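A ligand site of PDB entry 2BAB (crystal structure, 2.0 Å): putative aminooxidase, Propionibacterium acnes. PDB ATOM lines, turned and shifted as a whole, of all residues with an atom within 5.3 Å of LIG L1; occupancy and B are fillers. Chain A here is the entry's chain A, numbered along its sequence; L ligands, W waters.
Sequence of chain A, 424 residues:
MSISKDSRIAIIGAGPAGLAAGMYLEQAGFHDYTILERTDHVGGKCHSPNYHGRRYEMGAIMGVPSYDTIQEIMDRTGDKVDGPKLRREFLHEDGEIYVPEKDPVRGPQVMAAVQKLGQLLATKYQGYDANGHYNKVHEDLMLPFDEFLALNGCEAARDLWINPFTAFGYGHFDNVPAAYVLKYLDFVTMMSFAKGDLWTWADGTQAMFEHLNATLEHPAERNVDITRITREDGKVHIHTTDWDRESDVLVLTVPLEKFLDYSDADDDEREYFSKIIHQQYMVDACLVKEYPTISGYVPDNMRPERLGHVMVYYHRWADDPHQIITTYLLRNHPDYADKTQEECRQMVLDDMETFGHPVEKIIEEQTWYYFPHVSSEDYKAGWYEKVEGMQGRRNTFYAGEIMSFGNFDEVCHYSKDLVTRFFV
Water W1 lies within hydrogen-bond range of O1 of LIG L1 (2.5 Å), O of Leu 86 (3.0 Å) and NH1 of Arg 88 (3.3 Å).
The side-chain hydroxyl of Tyr 67 lies close to the side-chain amide oxygen of Asn 407. The backbone NH (N) of Tyr 328 sits at hydrogen-bond distance from the backbone carbonyl oxygen (O) of Val 312, 3.1 Å away. O of Arg 87 lies within hydrogen-bond range of N of Ser 295. The backbone carbonyl oxygen of Phe 168 sits at hydrogen-bond distance from the side-chain hydroxyl of Tyr 370 (2.6 Å). The side-chain hydroxyl (OH) of Tyr 184 is in hydrogen-bond range of the backbone carbonyl oxygen (O) of Pro 164, 2.7 Å away. OH of Tyr 170 lies close to OH of Tyr 370. O of Phe 193 lies within hydrogen-bond range of NH1 of Arg 88 (3.1 Å). The side-chain hydroxyl (OH) of Tyr 281 sits at hydrogen-bond distance from the backbone carbonyl oxygen (O) of Ala 167 (2.7 Å).
Ile 61 touches LIG L1 (CD1 to C6, 3.6 Å). Met 62 touches LIG L1. CG1 of Val 64 touches C18 of LIG L1, 3.7 Å away. OH of Tyr 67 touches C16 of LIG L1, 3.4 Å away. Leu 86 touches LIG L1 (CB to O1, 3.5 Å). Phe 168 touches LIG L1 (CD2 to C11, 3.2 Å). Tyr 170 touches LIG L1. OH of Tyr 184 touches C14 of LIG L1 (3.5 Å). Thr 189 touches LIG L1. CE1 of Phe 193 touches O2 of LIG L1, at 3.9 Å. Tyr 281 touches LIG L1. Ser 295 touches LIG L1 (CB to C2, 3.7 Å). CG2 of Val 312 touches C5 of LIG L1 (3.6 Å). Tyr 314 touches LIG L1 (CD1 to C4, 3.8 Å). Tyr 328 touches LIG L1. Tyr 370 touches LIG L1 (OH to C12, 3.7 Å). Hydrophobic or aromatic side chains that line LIG L1: Ile 61, Met 62, Val 64, Leu 86, Phe 168, Tyr 170, Tyr 184, Phe 193, Tyr 297, Val 312, Tyr 314 and Tyr 328. Of the 26 residues printed, 19 come within 4 Å of LIG L1.
An oxygen (O8) of LG2 L2 sits at hydrogen-bond distance from the backbone NH (N) of Met 62 (3.0 Å). The backbone carbonyl oxygen (O) of Met 62 lies within hydrogen-bond range of a nitrogen (N7) of LG2 L2, 2.8 Å away. OH of Tyr 67 is in hydrogen-bond range of O7 of LG2 L2, 2.8 Å away. N of Ile 61 lies within hydrogen-bond range of O8 of LG2 L2 (3.3 Å). OH of Tyr 297 is in hydrogen-bond range of O2 of LIG L1. An oxygen (O1) of LIG L1 is in hydrogen-bond range of the backbone NH of Arg 87. O2 of LIG L1 lies within salt-bridge range of NE of Arg 88 (3.0 Å). N of Asn 407 lies within hydrogen-bond range of O10 of LG2 L2 (3.2 Å).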
ATOM      1  N   ILE A  61     -29.930  32.898  18.425  1.00  0.00           N
ATOM      2  CA  ILE A  61     -31.033  32.478  19.311  1.00  0.00           C
ATOM      3  C   ILE A  61     -31.048  33.270  20.627  1.00  0.00           C
ATOM      4  O   ILE A  61     -32.133  33.648  21.125  1.00  0.00           O
ATOM      5  CB  ILE A  61     -30.860  30.984  19.677  1.00  0.00           C
ATOM      6  CG1 ILE A  61     -30.891  30.110  18.425  1.00  0.00           C
ATOM      7  CG2 ILE A  61     -31.903  30.543  20.708  1.00  0.00           C
ATOM      8  CD1 ILE A  61     -30.108  28.808  18.576  1.00  0.00           C
ATOM      9  N   MET A  62     -29.861  33.506  21.199  1.00  0.00           N
ATOM     10  CA  MET A  62     -29.780  33.833  22.605  1.00  0.00           C
ATOM     11  C   MET A  62     -28.768  34.920  22.994  1.00  0.00           C
ATOM     12  O   MET A  62     -27.883  35.313  22.228  1.00  0.00           O
ATOM     13  CB  MET A  62     -29.536  32.550  23.422  1.00  0.00           C
ATOM     14  CG  MET A  62     -28.097  32.071  23.434  1.00  0.00           C
ATOM     15  SD  MET A  62     -27.897  30.477  24.235  1.00  0.00           S
ATOM     16  CE  MET A  62     -28.606  29.384  22.999  1.00  0.00           C
ATOM     17  N   GLY A  63     -28.949  35.399  24.214  1.00  0.00           N
ATOM     18  CA  GLY A  63     -28.051  36.371  24.839  1.00  0.00           C
ATOM     19  C   GLY A  63     -27.884  36.047  26.317  1.00  0.00           C
ATOM     20  O   GLY A  63     -28.489  35.101  26.816  1.00  0.00           O
ATOM     21  N   VAL A  64     -27.064  36.842  26.998  1.00  0.00           N
ATOM     22  CA  VAL A  64     -26.913  36.748  28.457  1.00  0.00           C
ATOM     23  C   VAL A  64     -27.123  38.120  29.059  1.00  0.00           C
ATOM     24  O   VAL A  64     -27.045  39.120  28.342  1.00  0.00           O
ATOM     25  CB  VAL A  64     -25.507  36.190  28.887  1.00  0.00           C
ATOM     26  CG1 VAL A  64     -25.374  34.691  28.571  1.00  0.00           C
ATOM     27  CG2 VAL A  64     -24.370  36.994  28.280  1.00  0.00           C
ATOM     28  N   TYR A  67     -25.156  41.258  28.100  1.00  0.00           N
ATOM     29  CA  TYR A  67     -25.290  41.819  26.736  1.00  0.00           C
ATOM     30  C   TYR A  67     -25.768  43.292  26.815  1.00  0.00           C
ATOM     31  O   TYR A  67     -26.873  43.625  26.366  1.00  0.00           O
ATOM     32  CB  TYR A  67     -26.290  40.977  25.900  1.00  0.00           C
ATOM     33  CG  TYR A  67     -25.683  39.852  25.097  1.00  0.00           C
ATOM     34  CD1 TYR A  67     -24.485  39.241  25.458  1.00  0.00           C
ATOM     35  CD2 TYR A  67     -26.343  39.362  23.966  1.00  0.00           C
ATOM     36  CE1 TYR A  67     -23.934  38.212  24.689  1.00  0.00           C
ATOM     37  CE2 TYR A  67     -25.791  38.323  23.184  1.00  0.00           C
ATOM     38  CZ  TYR A  67     -24.590  37.744  23.563  1.00  0.00           C
ATOM     39  OH  TYR A  67     -24.033  36.726  22.786  1.00  0.00           O
ATOM     40  N   LEU A  86     -34.850  28.321  27.778  1.00  0.00           N
ATOM     41  CA  LEU A  86     -33.943  27.294  27.298  1.00  0.00           C
ATOM     42  C   LEU A  86     -33.696  26.249  28.399  1.00  0.00           C
ATOM     43  O   LEU A  86     -33.475  26.603  29.564  1.00  0.00           O
ATOM     44  CB  LEU A  86     -32.633  27.915  26.887  1.00  0.00           C
ATOM     45  CG  LEU A  86     -32.695  28.799  25.638  1.00  0.00           C
ATOM     46  CD1 LEU A  86     -31.401  29.594  25.503  1.00  0.00           C
ATOM     47  CD2 LEU A  86     -32.938  27.958  24.387  1.00  0.00           C
ATOM     48  N   ARG A  87     -33.743  24.985  28.025  1.00  0.00           N
ATOM     49  CA  ARG A  87     -33.452  23.888  28.940  1.00  0.00           C
ATOM     50  C   ARG A  87     -32.709  22.806  28.192  1.00  0.00           C
ATOM     51  O   ARG A  87     -32.955  22.588  27.008  1.00  0.00           O
ATOM     52  CB  ARG A  87     -34.738  23.349  29.550  1.00  0.00           C
ATOM     53  CG  ARG A  87     -35.497  24.330  30.434  1.00  0.00           C
ATOM     54  CD  ARG A  87     -36.830  23.716  30.851  1.00  0.00           C
ATOM     55  NE  ARG A  87     -37.679  24.569  31.681  1.00  0.00           N
ATOM     56  CZ  ARG A  87     -37.531  24.775  32.993  1.00  0.00           C
ATOM     57  NH1 ARG A  87     -36.502  24.251  33.670  1.00  0.00           N
ATOM     58  NH2 ARG A  87     -38.417  25.536  33.639  1.00  0.00           N
ATOM     59  N   ARG A  88     -31.789  22.137  28.880  1.00  0.00           N
ATOM     60  CA  ARG A  88     -30.853  21.211  28.249  1.00  0.00           C
ATOM     61  C   ARG A  88     -30.670  19.905  29.004  1.00  0.00           C
ATOM     62  O   ARG A  88     -30.664  19.882  30.234  1.00  0.00           O
ATOM     63  CB  ARG A  88     -29.461  21.854  28.079  1.00  0.00           C
ATOM     64  CG  ARG A  88     -28.681  22.082  29.391  1.00  0.00           C
ATOM     65  CD  ARG A  88     -27.323  22.716  29.171  1.00  0.00           C
ATOM     66  NE  ARG A  88     -27.450  24.128  28.849  1.00  0.00           N
ATOM     67  CZ  ARG A  88     -27.067  25.157  29.610  1.00  0.00           C
ATOM     68  NH1 ARG A  88     -27.285  26.396  29.174  1.00  0.00           N
ATOM     69  NH2 ARG A  88     -26.471  24.995  30.804  1.00  0.00           N
ATOM     70  N   PRO A 164     -20.941  25.640  25.198  1.00  0.00           N
ATOM     71  CA  PRO A 164     -21.372  26.823  24.444  1.00  0.00           C
ATOM     72  C   PRO A 164     -20.337  27.387  23.452  1.00  0.00           C
ATOM     73  O   PRO A 164     -20.468  28.504  22.999  1.00  0.00           O
ATOM     74  CB  PRO A 164     -21.657  27.835  25.552  1.00  0.00           C
ATOM     75  CG  PRO A 164     -20.640  27.502  26.582  1.00  0.00           C
ATOM     76  CD  PRO A 164     -20.432  26.026  26.528  1.00  0.00           C
ATOM     77  N   ALA A 167     -19.918  23.277  20.192  1.00  0.00           N
ATOM     78  CA  ALA A 167     -21.277  22.941  19.769  1.00  0.00           C
ATOM     79  C   ALA A 167     -21.947  24.151  19.101  1.00  0.00           C
ATOM     80  O   ALA A 167     -22.785  23.981  18.188  1.00  0.00           O
ATOM     81  CB  ALA A 167     -22.095  22.463  20.956  1.00  0.00           C
ATOM     82  N   PHE A 168     -21.542  25.345  19.522  1.00  0.00           N
ATOM     83  CA  PHE A 168     -22.098  26.607  19.044  1.00  0.00           C
ATOM     84  C   PHE A 168     -21.364  27.130  17.802  1.00  0.00           C
ATOM     85  O   PHE A 168     -21.515  28.291  17.416  1.00  0.00           O
ATOM     86  CB  PHE A 168     -22.067  27.651  20.161  1.00  0.00           C
ATOM     87  CG  PHE A 168     -23.153  27.480  21.218  1.00  0.00           C
ATOM     88  CD1 PHE A 168     -23.868  26.296  21.366  1.00  0.00           C
ATOM     89  CD2 PHE A 168     -23.429  28.534  22.095  1.00  0.00           C
ATOM     90  CE1 PHE A 168     -24.870  26.192  22.355  1.00  0.00           C
ATOM     91  CE2 PHE A 168     -24.408  28.421  23.078  1.00  0.00           C
ATOM     92  CZ  PHE A 168     -25.133  27.255  23.203  1.00  0.00           C
ATOM     93  N   TYR A 170     -18.117  27.514  17.006  1.00  0.00           N
ATOM     94  CA  TYR A 170     -16.938  28.368  17.013  1.00  0.00           C
ATOM     95  C   TYR A 170     -15.610  27.595  16.844  1.00  0.00           C
ATOM     96  O   TYR A 170     -14.562  28.202  16.778  1.00  0.00           O
ATOM     97  CB  TYR A 170     -16.918  29.220  18.268  1.00  0.00           C
ATOM     98  CG  TYR A 170     -18.054  30.214  18.371  1.00  0.00           C
ATOM     99  CD1 TYR A 170     -18.147  31.268  17.484  1.00  0.00           C
ATOM    100  CD2 TYR A 170     -19.013  30.107  19.375  1.00  0.00           C
ATOM    101  CE1 TYR A 170     -19.174  32.195  17.581  1.00  0.00           C
ATOM    102  CE2 TYR A 170     -20.040  31.035  19.486  1.00  0.00           C
ATOM    103  CZ  TYR A 170     -20.109  32.071  18.594  1.00  0.00           C
ATOM    104  OH  TYR A 170     -21.112  32.972  18.701  1.00  0.00           O
ATOM    105  N   TYR A 184     -15.523  36.075  24.369  1.00  0.00           N
ATOM    106  CA  TYR A 184     -16.892  35.582  24.257  1.00  0.00           C
ATOM    107  C   TYR A 184     -17.338  35.035  25.603  1.00  0.00           C
ATOM    108  O   TYR A 184     -18.140  35.648  26.284  1.00  0.00           O
ATOM    109  CB  TYR A 184     -16.984  34.512  23.162  1.00  0.00           C
ATOM    110  CG  TYR A 184     -18.188  33.580  23.225  1.00  0.00           C
ATOM    111  CD1 TYR A 184     -19.431  34.015  23.681  1.00  0.00           C
ATOM    112  CD2 TYR A 184     -18.072  32.263  22.801  1.00  0.00           C
ATOM    113  CE1 TYR A 184     -20.511  33.170  23.732  1.00  0.00           C
ATOM    114  CE2 TYR A 184     -19.149  31.397  22.853  1.00  0.00           C
ATOM    115  CZ  TYR A 184     -20.365  31.845  23.308  1.00  0.00           C
ATOM    116  OH  TYR A 184     -21.426  30.962  23.362  1.00  0.00           O
ATOM    117  N   LEU A 185     -16.803  33.883  25.980  1.00  0.00           N
ATOM    118  CA  LEU A 185     -17.112  33.277  27.263  1.00  0.00           C
ATOM    119  C   LEU A 185     -16.170  33.791  28.368  1.00  0.00           C
ATOM    120  O   LEU A 185     -15.346  33.043  28.884  1.00  0.00           O
ATOM    121  CB  LEU A 185     -17.047  31.747  27.148  1.00  0.00           C
ATOM    122  CG  LEU A 185     -18.124  31.114  26.271  1.00  0.00           C
ATOM    123  CD1 LEU A 185     -17.679  29.742  25.665  1.00  0.00           C
ATOM    124  CD2 LEU A 185     -19.441  30.969  27.039  1.00  0.00           C
ATOM    125  N   THR A 189     -20.066  35.582  31.608  1.00  0.00           N
ATOM    126  CA  THR A 189     -20.840  34.981  30.527  1.00  0.00           C
ATOM    127  C   THR A 189     -20.911  33.456  30.686  1.00  0.00           C
ATOM    128  O   THR A 189     -22.006  32.889  30.577  1.00  0.00           O
ATOM    129  CB  THR A 189     -20.291  35.395  29.136  1.00  0.00           C
ATOM    130  OG1 THR A 189     -20.279  36.835  29.026  1.00  0.00           O
ATOM    131  CG2 THR A 189     -21.127  34.780  27.992  1.00  0.00           C
ATOM    132  N   PHE A 193     -24.402  31.180  31.279  1.00  0.00           N
ATOM    133  CA  PHE A 193     -24.727  30.032  30.458  1.00  0.00           C
ATOM    134  C   PHE A 193     -24.905  28.812  31.349  1.00  0.00           C
ATOM    135  O   PHE A 193     -25.916  28.146  31.264  1.00  0.00           O
ATOM    136  CB  PHE A 193     -23.678  29.729  29.371  1.00  0.00           C
ATOM    137  CG  PHE A 193     -23.998  28.484  28.579  1.00  0.00           C
ATOM    138  CD1 PHE A 193     -24.856  28.530  27.498  1.00  0.00           C
ATOM    139  CD2 PHE A 193     -23.472  27.239  28.956  1.00  0.00           C
ATOM    140  CE1 PHE A 193     -25.168  27.384  26.790  1.00  0.00           C
ATOM    141  CE2 PHE A 193     -23.798  26.093  28.263  1.00  0.00           C
ATOM    142  CZ  PHE A 193     -24.638  26.162  27.187  1.00  0.00           C
ATOM    143  N   LEU A 198     -30.390  32.870  30.275  1.00  0.00           N
ATOM    144  CA  LEU A 198     -30.194  33.094  28.860  1.00  0.00           C
ATOM    145  C   LEU A 198     -31.414  33.771  28.237  1.00  0.00           C
ATOM    146  O   LEU A 198     -32.540  33.267  28.329  1.00  0.00           O
ATOM    147  CB  LEU A 198     -29.926  31.771  28.147  1.00  0.00           C
ATOM    148  CG  LEU A 198     -28.595  31.076  28.510  1.00  0.00           C
ATOM    149  CD1 LEU A 198     -28.613  29.587  28.184  1.00  0.00           C
ATOM    150  CD2 LEU A 198     -27.428  31.766  27.828  1.00  0.00           C
ATOM    151  N   TYR A 281     -20.547  26.307   9.552  1.00  0.00           N
ATOM    152  CA  TYR A 281     -21.493  25.888  10.568  1.00  0.00           C
ATOM    153  C   TYR A 281     -22.854  25.623   9.919  1.00  0.00           C
ATOM    154  O   TYR A 281     -23.486  26.536   9.391  1.00  0.00           O
ATOM    155  CB  TYR A 281     -21.599  27.000  11.621  1.00  0.00           C
ATOM    156  CG  TYR A 281     -22.268  26.633  12.935  1.00  0.00           C
ATOM    157  CD1 TYR A 281     -22.187  25.345  13.473  1.00  0.00           C
ATOM    158  CD2 TYR A 281     -22.928  27.625  13.677  1.00  0.00           C
ATOM    159  CE1 TYR A 281     -22.778  25.041  14.697  1.00  0.00           C
ATOM    160  CE2 TYR A 281     -23.514  27.331  14.894  1.00  0.00           C
ATOM    161  CZ  TYR A 281     -23.433  26.051  15.403  1.00  0.00           C
ATOM    162  OH  TYR A 281     -24.010  25.748  16.613  1.00  0.00           O
ATOM    163  N   SER A 295     -33.841  20.524  24.994  1.00  0.00           N
ATOM    164  CA  SER A 295     -32.742  20.593  24.031  1.00  0.00           C
ATOM    165  C   SER A 295     -31.660  19.565  24.440  1.00  0.00           C
ATOM    166  O   SER A 295     -31.577  19.173  25.604  1.00  0.00           O
ATOM    167  CB  SER A 295     -32.135  22.002  23.954  1.00  0.00           C
ATOM    168  OG  SER A 295     -33.079  22.955  23.539  1.00  0.00           O
ATOM    169  N   TYR A 297     -27.444  18.363  24.072  1.00  0.00           N
ATOM    170  CA  TYR A 297     -26.048  18.599  23.759  1.00  0.00           C
ATOM    171  C   TYR A 297     -25.303  17.268  23.743  1.00  0.00           C
ATOM    172  O   TYR A 297     -25.609  16.377  24.546  1.00  0.00           O
ATOM    173  CB  TYR A 297     -25.385  19.450  24.852  1.00  0.00           C
ATOM    174  CG  TYR A 297     -25.719  20.915  24.849  1.00  0.00           C
ATOM    175  CD1 TYR A 297     -24.779  21.855  24.476  1.00  0.00           C
ATOM    176  CD2 TYR A 297     -26.978  21.365  25.275  1.00  0.00           C
ATOM    177  CE1 TYR A 297     -25.077  23.203  24.476  1.00  0.00           C
ATOM    178  CE2 TYR A 297     -27.284  22.722  25.281  1.00  0.00           C
ATOM    179  CZ  TYR A 297     -26.325  23.633  24.883  1.00  0.00           C
ATOM    180  OH  TYR A 297     -26.566  24.979  24.898  1.00  0.00           O
ATOM    181  N   VAL A 312     -25.557  19.588  18.975  1.00  0.00           N
ATOM    182  CA  VAL A 312     -26.601  20.191  19.781  1.00  0.00           C
ATOM    183  C   VAL A 312     -27.840  20.303  18.874  1.00  0.00           C
ATOM    184  O   VAL A 312     -27.704  20.385  17.648  1.00  0.00           O
ATOM    185  CB  VAL A 312     -26.148  21.566  20.357  1.00  0.00           C
ATOM    186  CG1 VAL A 312     -25.883  22.565  19.232  1.00  0.00           C
ATOM    187  CG2 VAL A 312     -27.179  22.117  21.360  1.00  0.00           C
ATOM    188  N   TYR A 313     -29.024  20.241  19.465  1.00  0.00           N
ATOM    189  CA  TYR A 313     -30.269  20.562  18.746  1.00  0.00           C
ATOM    190  C   TYR A 313     -31.176  21.365  19.671  1.00  0.00           C
ATOM    191  O   TYR A 313     -31.105  21.229  20.891  1.00  0.00           O
ATOM    192  CB  TYR A 313     -30.951  19.299  18.185  1.00  0.00           C
ATOM    193  CG  TYR A 313     -31.265  18.246  19.215  1.00  0.00           C
ATOM    194  CD1 TYR A 313     -32.424  18.313  19.981  1.00  0.00           C
ATOM    195  CD2 TYR A 313     -30.395  17.154  19.435  1.00  0.00           C
ATOM    196  CE1 TYR A 313     -32.714  17.348  20.940  1.00  0.00           C
ATOM    197  CE2 TYR A 313     -30.670  16.180  20.395  1.00  0.00           C
ATOM    198  CZ  TYR A 313     -31.819  16.277  21.130  1.00  0.00           C
ATOM    199  OH  TYR A 313     -32.104  15.331  22.081  1.00  0.00           O
ATOM    200  N   TYR A 314     -32.031  22.191  19.056  1.00  0.00           N
ATOM    201  CA  TYR A 314     -32.751  23.262  19.755  1.00  0.00           C
ATOM    202  C   TYR A 314     -34.239  22.971  19.816  1.00  0.00           C
ATOM    203  O   TYR A 314     -34.938  23.045  18.813  1.00  0.00           O
ATOM    204  CB  TYR A 314     -32.453  24.596  19.062  1.00  0.00           C
ATOM    205  CG  TYR A 314     -33.174  25.844  19.583  1.00  0.00           C
ATOM    206  CD1 TYR A 314     -33.653  25.927  20.896  1.00  0.00           C
ATOM    207  CD2 TYR A 314     -33.353  26.952  18.754  1.00  0.00           C
ATOM    208  CE1 TYR A 314     -34.297  27.079  21.363  1.00  0.00           C
ATOM    209  CE2 TYR A 314     -34.007  28.122  19.212  1.00  0.00           C
ATOM    210  CZ  TYR A 314     -34.486  28.163  20.507  1.00  0.00           C
ATOM    211  OH  TYR A 314     -35.133  29.275  20.984  1.00  0.00           O
ATOM    212  N   TYR A 328     -27.402  21.354  14.750  1.00  0.00           N
ATOM    213  CA  TYR A 328     -26.152  22.108  14.554  1.00  0.00           C
ATOM    214  C   TYR A 328     -24.932  21.182  14.424  1.00  0.00           C
ATOM    215  O   TYR A 328     -24.725  20.291  15.264  1.00  0.00           O
ATOM    216  CB  TYR A 328     -25.922  23.100  15.714  1.00  0.00           C
ATOM    217  CG  TYR A 328     -27.090  24.015  15.881  1.00  0.00           C
ATOM    218  CD1 TYR A 328     -27.089  25.270  15.297  1.00  0.00           C
ATOM    219  CD2 TYR A 328     -28.243  23.599  16.547  1.00  0.00           C
ATOM    220  CE1 TYR A 328     -28.204  26.106  15.415  1.00  0.00           C
ATOM    221  CE2 TYR A 328     -29.350  24.425  16.644  1.00  0.00           C
ATOM    222  CZ  TYR A 328     -29.327  25.675  16.096  1.00  0.00           C
ATOM    223  OH  TYR A 328     -30.445  26.479  16.196  1.00  0.00           O
ATOM    224  N   TYR A 370     -19.225  31.523   9.227  1.00  0.00           N
ATOM    225  CA  TYR A 370     -19.352  31.644  10.670  1.00  0.00           C
ATOM    226  C   TYR A 370     -17.995  31.938  11.303  1.00  0.00           C
ATOM    227  O   TYR A 370     -16.987  31.384  10.875  1.00  0.00           O
ATOM    228  CB  TYR A 370     -19.953  30.338  11.214  1.00  0.00           C
ATOM    229  CG  TYR A 370     -20.493  30.451  12.609  1.00  0.00           C
ATOM    230  CD1 TYR A 370     -21.663  31.161  12.865  1.00  0.00           C
ATOM    231  CD2 TYR A 370     -19.864  29.817  13.674  1.00  0.00           C
ATOM    232  CE1 TYR A 370     -22.179  31.256  14.141  1.00  0.00           C
ATOM    233  CE2 TYR A 370     -20.364  29.905  14.951  1.00  0.00           C
ATOM    234  CZ  TYR A 370     -21.528  30.623  15.185  1.00  0.00           C
ATOM    235  OH  TYR A 370     -22.027  30.701  16.463  1.00  0.00           O
ATOM    236  N   ASN A 407     -20.397  37.008  17.951  1.00  0.00           N
ATOM    237  CA  ASN A 407     -21.718  37.002  18.579  1.00  0.00           C
ATOM    238  C   ASN A 407     -22.278  38.395  18.443  1.00  0.00           C
ATOM    239  O   ASN A 407     -21.501  39.333  18.175  1.00  0.00           O
ATOM    240  CB  ASN A 407     -21.737  36.407  20.014  1.00  0.00           C
ATOM    241  CG  ASN A 407     -21.251  37.357  21.117  1.00  0.00           C
ATOM    242  OD1 ASN A 407     -21.612  38.531  21.188  1.00  0.00           O
ATOM    243  ND2 ASN A 407     -20.523  36.786  22.057  1.00  0.00           N
HETATM  244  O1  LIG L   1     -30.410  25.251  27.482  1.00  0.00           O
HETATM  245  C1  LIG L   1     -29.776  25.330  26.405  1.00  0.00           C
HETATM  246  O2  LIG L   1     -28.550  25.552  26.417  1.00  0.00           O
HETATM  247  C2  LIG L   1     -30.490  25.150  25.076  1.00  0.00           C
HETATM  248  C3  LIG L   1     -29.604  25.547  23.897  1.00  0.00           C
HETATM  249  C4  LIG L   1     -30.273  25.349  22.528  1.00  0.00           C
HETATM  250  C5  LIG L   1     -29.277  25.065  21.388  1.00  0.00           C
HETATM  251  C6  LIG L   1     -28.730  26.351  20.817  1.00  0.00           C
HETATM  252  C7  LIG L   1     -27.649  26.287  19.744  1.00  0.00           C
HETATM  253  C8  LIG L   1     -26.829  27.596  19.835  1.00  0.00           C
HETATM  254  C9  LIG L   1     -25.996  27.900  18.600  1.00  0.00           C
HETATM  255  C10 LIG L   1     -25.039  29.087  18.696  1.00  0.00           C
HETATM  256  C11 LIG L   1     -24.907  29.963  19.708  1.00  0.00           C
HETATM  257  C12 LIG L   1     -23.914  31.043  19.579  1.00  0.00           C
HETATM  258  C13 LIG L   1     -23.672  32.005  20.493  1.00  0.00           C
HETATM  259  C14 LIG L   1     -24.400  32.088  21.825  1.00  0.00           C
HETATM  260  C15 LIG L   1     -23.975  33.343  22.567  1.00  0.00           C
HETATM  261  C16 LIG L   1     -24.690  33.600  23.905  1.00  0.00           C
HETATM  262  C17 LIG L   1     -24.729  32.404  24.866  1.00  0.00           C
HETATM  263  C18 LIG L   1     -23.746  32.503  26.021  1.00  0.00           C
HETATM  264  P1  LG2 L   2     -23.695  39.334   9.832  1.00  0.00           P
HETATM  265  O1  LG2 L   2     -24.790  38.962  10.799  1.00  0.00           O
HETATM  266  O2  LG2 L   2     -23.157  38.187   9.001  1.00  0.00           O
HETATM  267  O3  LG2 L   2     -24.251  40.445   8.791  1.00  0.00           O
HETATM  268  C1  LG2 L   2     -23.537  40.739   7.619  1.00  0.00           C
HETATM  269  C2  LG2 L   2     -24.444  41.531   6.693  1.00  0.00           C
HETATM  270  O4  LG2 L   2     -23.718  42.056   5.600  1.00  0.00           O
HETATM  271  C3  LG2 L   2     -25.554  40.650   6.157  1.00  0.00           C
HETATM  272  O5  LG2 L   2     -26.772  41.353   6.178  1.00  0.00           O
HETATM  273  C4  LG2 L   2     -25.076  40.356   4.748  1.00  0.00           C
HETATM  274  O6  LG2 L   2     -26.154  40.059   3.899  1.00  0.00           O
HETATM  275  C5  LG2 L   2     -24.346  41.655   4.391  1.00  0.00           C
HETATM  276  N1  LG2 L   2     -23.358  41.538   3.322  1.00  0.00           N
HETATM  277  C6  LG2 L   2     -22.433  40.527   3.117  1.00  0.00           C
HETATM  278  N2  LG2 L   2     -21.708  40.838   2.001  1.00  0.00           N
HETATM  279  C7  LG2 L   2     -22.147  42.022   1.509  1.00  0.00           C
HETATM  280  C8  LG2 L   2     -21.760  42.796   0.411  1.00  0.00           C
HETATM  281  N3  LG2 L   2     -20.910  42.321  -0.501  1.00  0.00           N
HETATM  282  N4  LG2 L   2     -22.421  43.984   0.165  1.00  0.00           N
HETATM  283  C9  LG2 L   2     -23.444  44.421   1.014  1.00  0.00           C
HETATM  284  N5  LG2 L   2     -23.831  43.656   2.096  1.00  0.00           N
HETATM  285  C10 LG2 L   2     -23.192  42.475   2.335  1.00  0.00           C
HETATM  286  N6  LG2 L   2     -24.834  35.317  18.325  1.00  0.00           N
HETATM  287  C11 LG2 L   2     -25.294  35.530  19.591  1.00  0.00           C
HETATM  288  O7  LG2 L   2     -24.997  36.573  20.180  1.00  0.00           O
HETATM  289  N7  LG2 L   2     -26.121  34.594  20.193  1.00  0.00           N
HETATM  290  C12 LG2 L   2     -26.456  33.412  19.559  1.00  0.00           C
HETATM  291  O8  LG2 L   2     -27.184  32.579  20.153  1.00  0.00           O
HETATM  292  C13 LG2 L   2     -25.965  33.171  18.281  1.00  0.00           C
HETATM  293  N8  LG2 L   2     -26.212  31.968  17.635  1.00  0.00           N
HETATM  294  C14 LG2 L   2     -25.904  31.830  16.303  1.00  0.00           C
HETATM  295  C15 LG2 L   2     -26.316  30.684  15.622  1.00  0.00           C
HETATM  296  C16 LG2 L   2     -26.095  30.552  14.260  1.00  0.00           C
HETATM  297  C17 LG2 L   2     -26.552  29.325  13.529  1.00  0.00           C
HETATM  298  C18 LG2 L   2     -25.472  31.586  13.583  1.00  0.00           C
HETATM  299  C19 LG2 L   2     -25.203  31.471  12.099  1.00  0.00           C
HETATM  300  C20 LG2 L   2     -25.053  32.724  14.272  1.00  0.00           C
HETATM  301  C21 LG2 L   2     -25.261  32.868  15.634  1.00  0.00           C
HETATM  302  N9  LG2 L   2     -24.773  33.968  16.362  1.00  0.00           N
HETATM  303  C22 LG2 L   2     -25.170  34.142  17.662  1.00  0.00           C
HETATM  304  C23 LG2 L   2     -23.787  34.950  15.823  1.00  0.00           C
HETATM  305  C24 LG2 L   2     -24.458  36.265  15.430  1.00  0.00           C
HETATM  306  O9  LG2 L   2     -25.633  36.004  14.669  1.00  0.00           O
HETATM  307  C25 LG2 L   2     -23.450  37.083  14.593  1.00  0.00           C
HETATM  308  O10 LG2 L   2     -22.235  37.213  15.302  1.00  0.00           O
HETATM  309  C26 LG2 L   2     -23.953  38.482  14.217  1.00  0.00           C
HETATM  310  O11 LG2 L   2     -25.137  38.390  13.441  1.00  0.00           O
HETATM  311  C27 LG2 L   2     -22.831  39.190  13.462  1.00  0.00           C
HETATM  312  O12 LG2 L   2     -23.297  40.421  12.959  1.00  0.00           O
HETATM  313  P2  LG2 L   2     -22.532  41.143  11.744  1.00  0.00           P
HETATM  314  O13 LG2 L   2     -23.352  42.345  11.323  1.00  0.00           O
HETATM  315  O14 LG2 L   2     -21.095  41.484  12.104  1.00  0.00           O
HETATM  316  O15 LG2 L   2     -22.449  40.039  10.584  1.00  0.00           O
HETATM  317  O   HOH W   1     -30.508  26.382  29.668  1.00  0.00           O
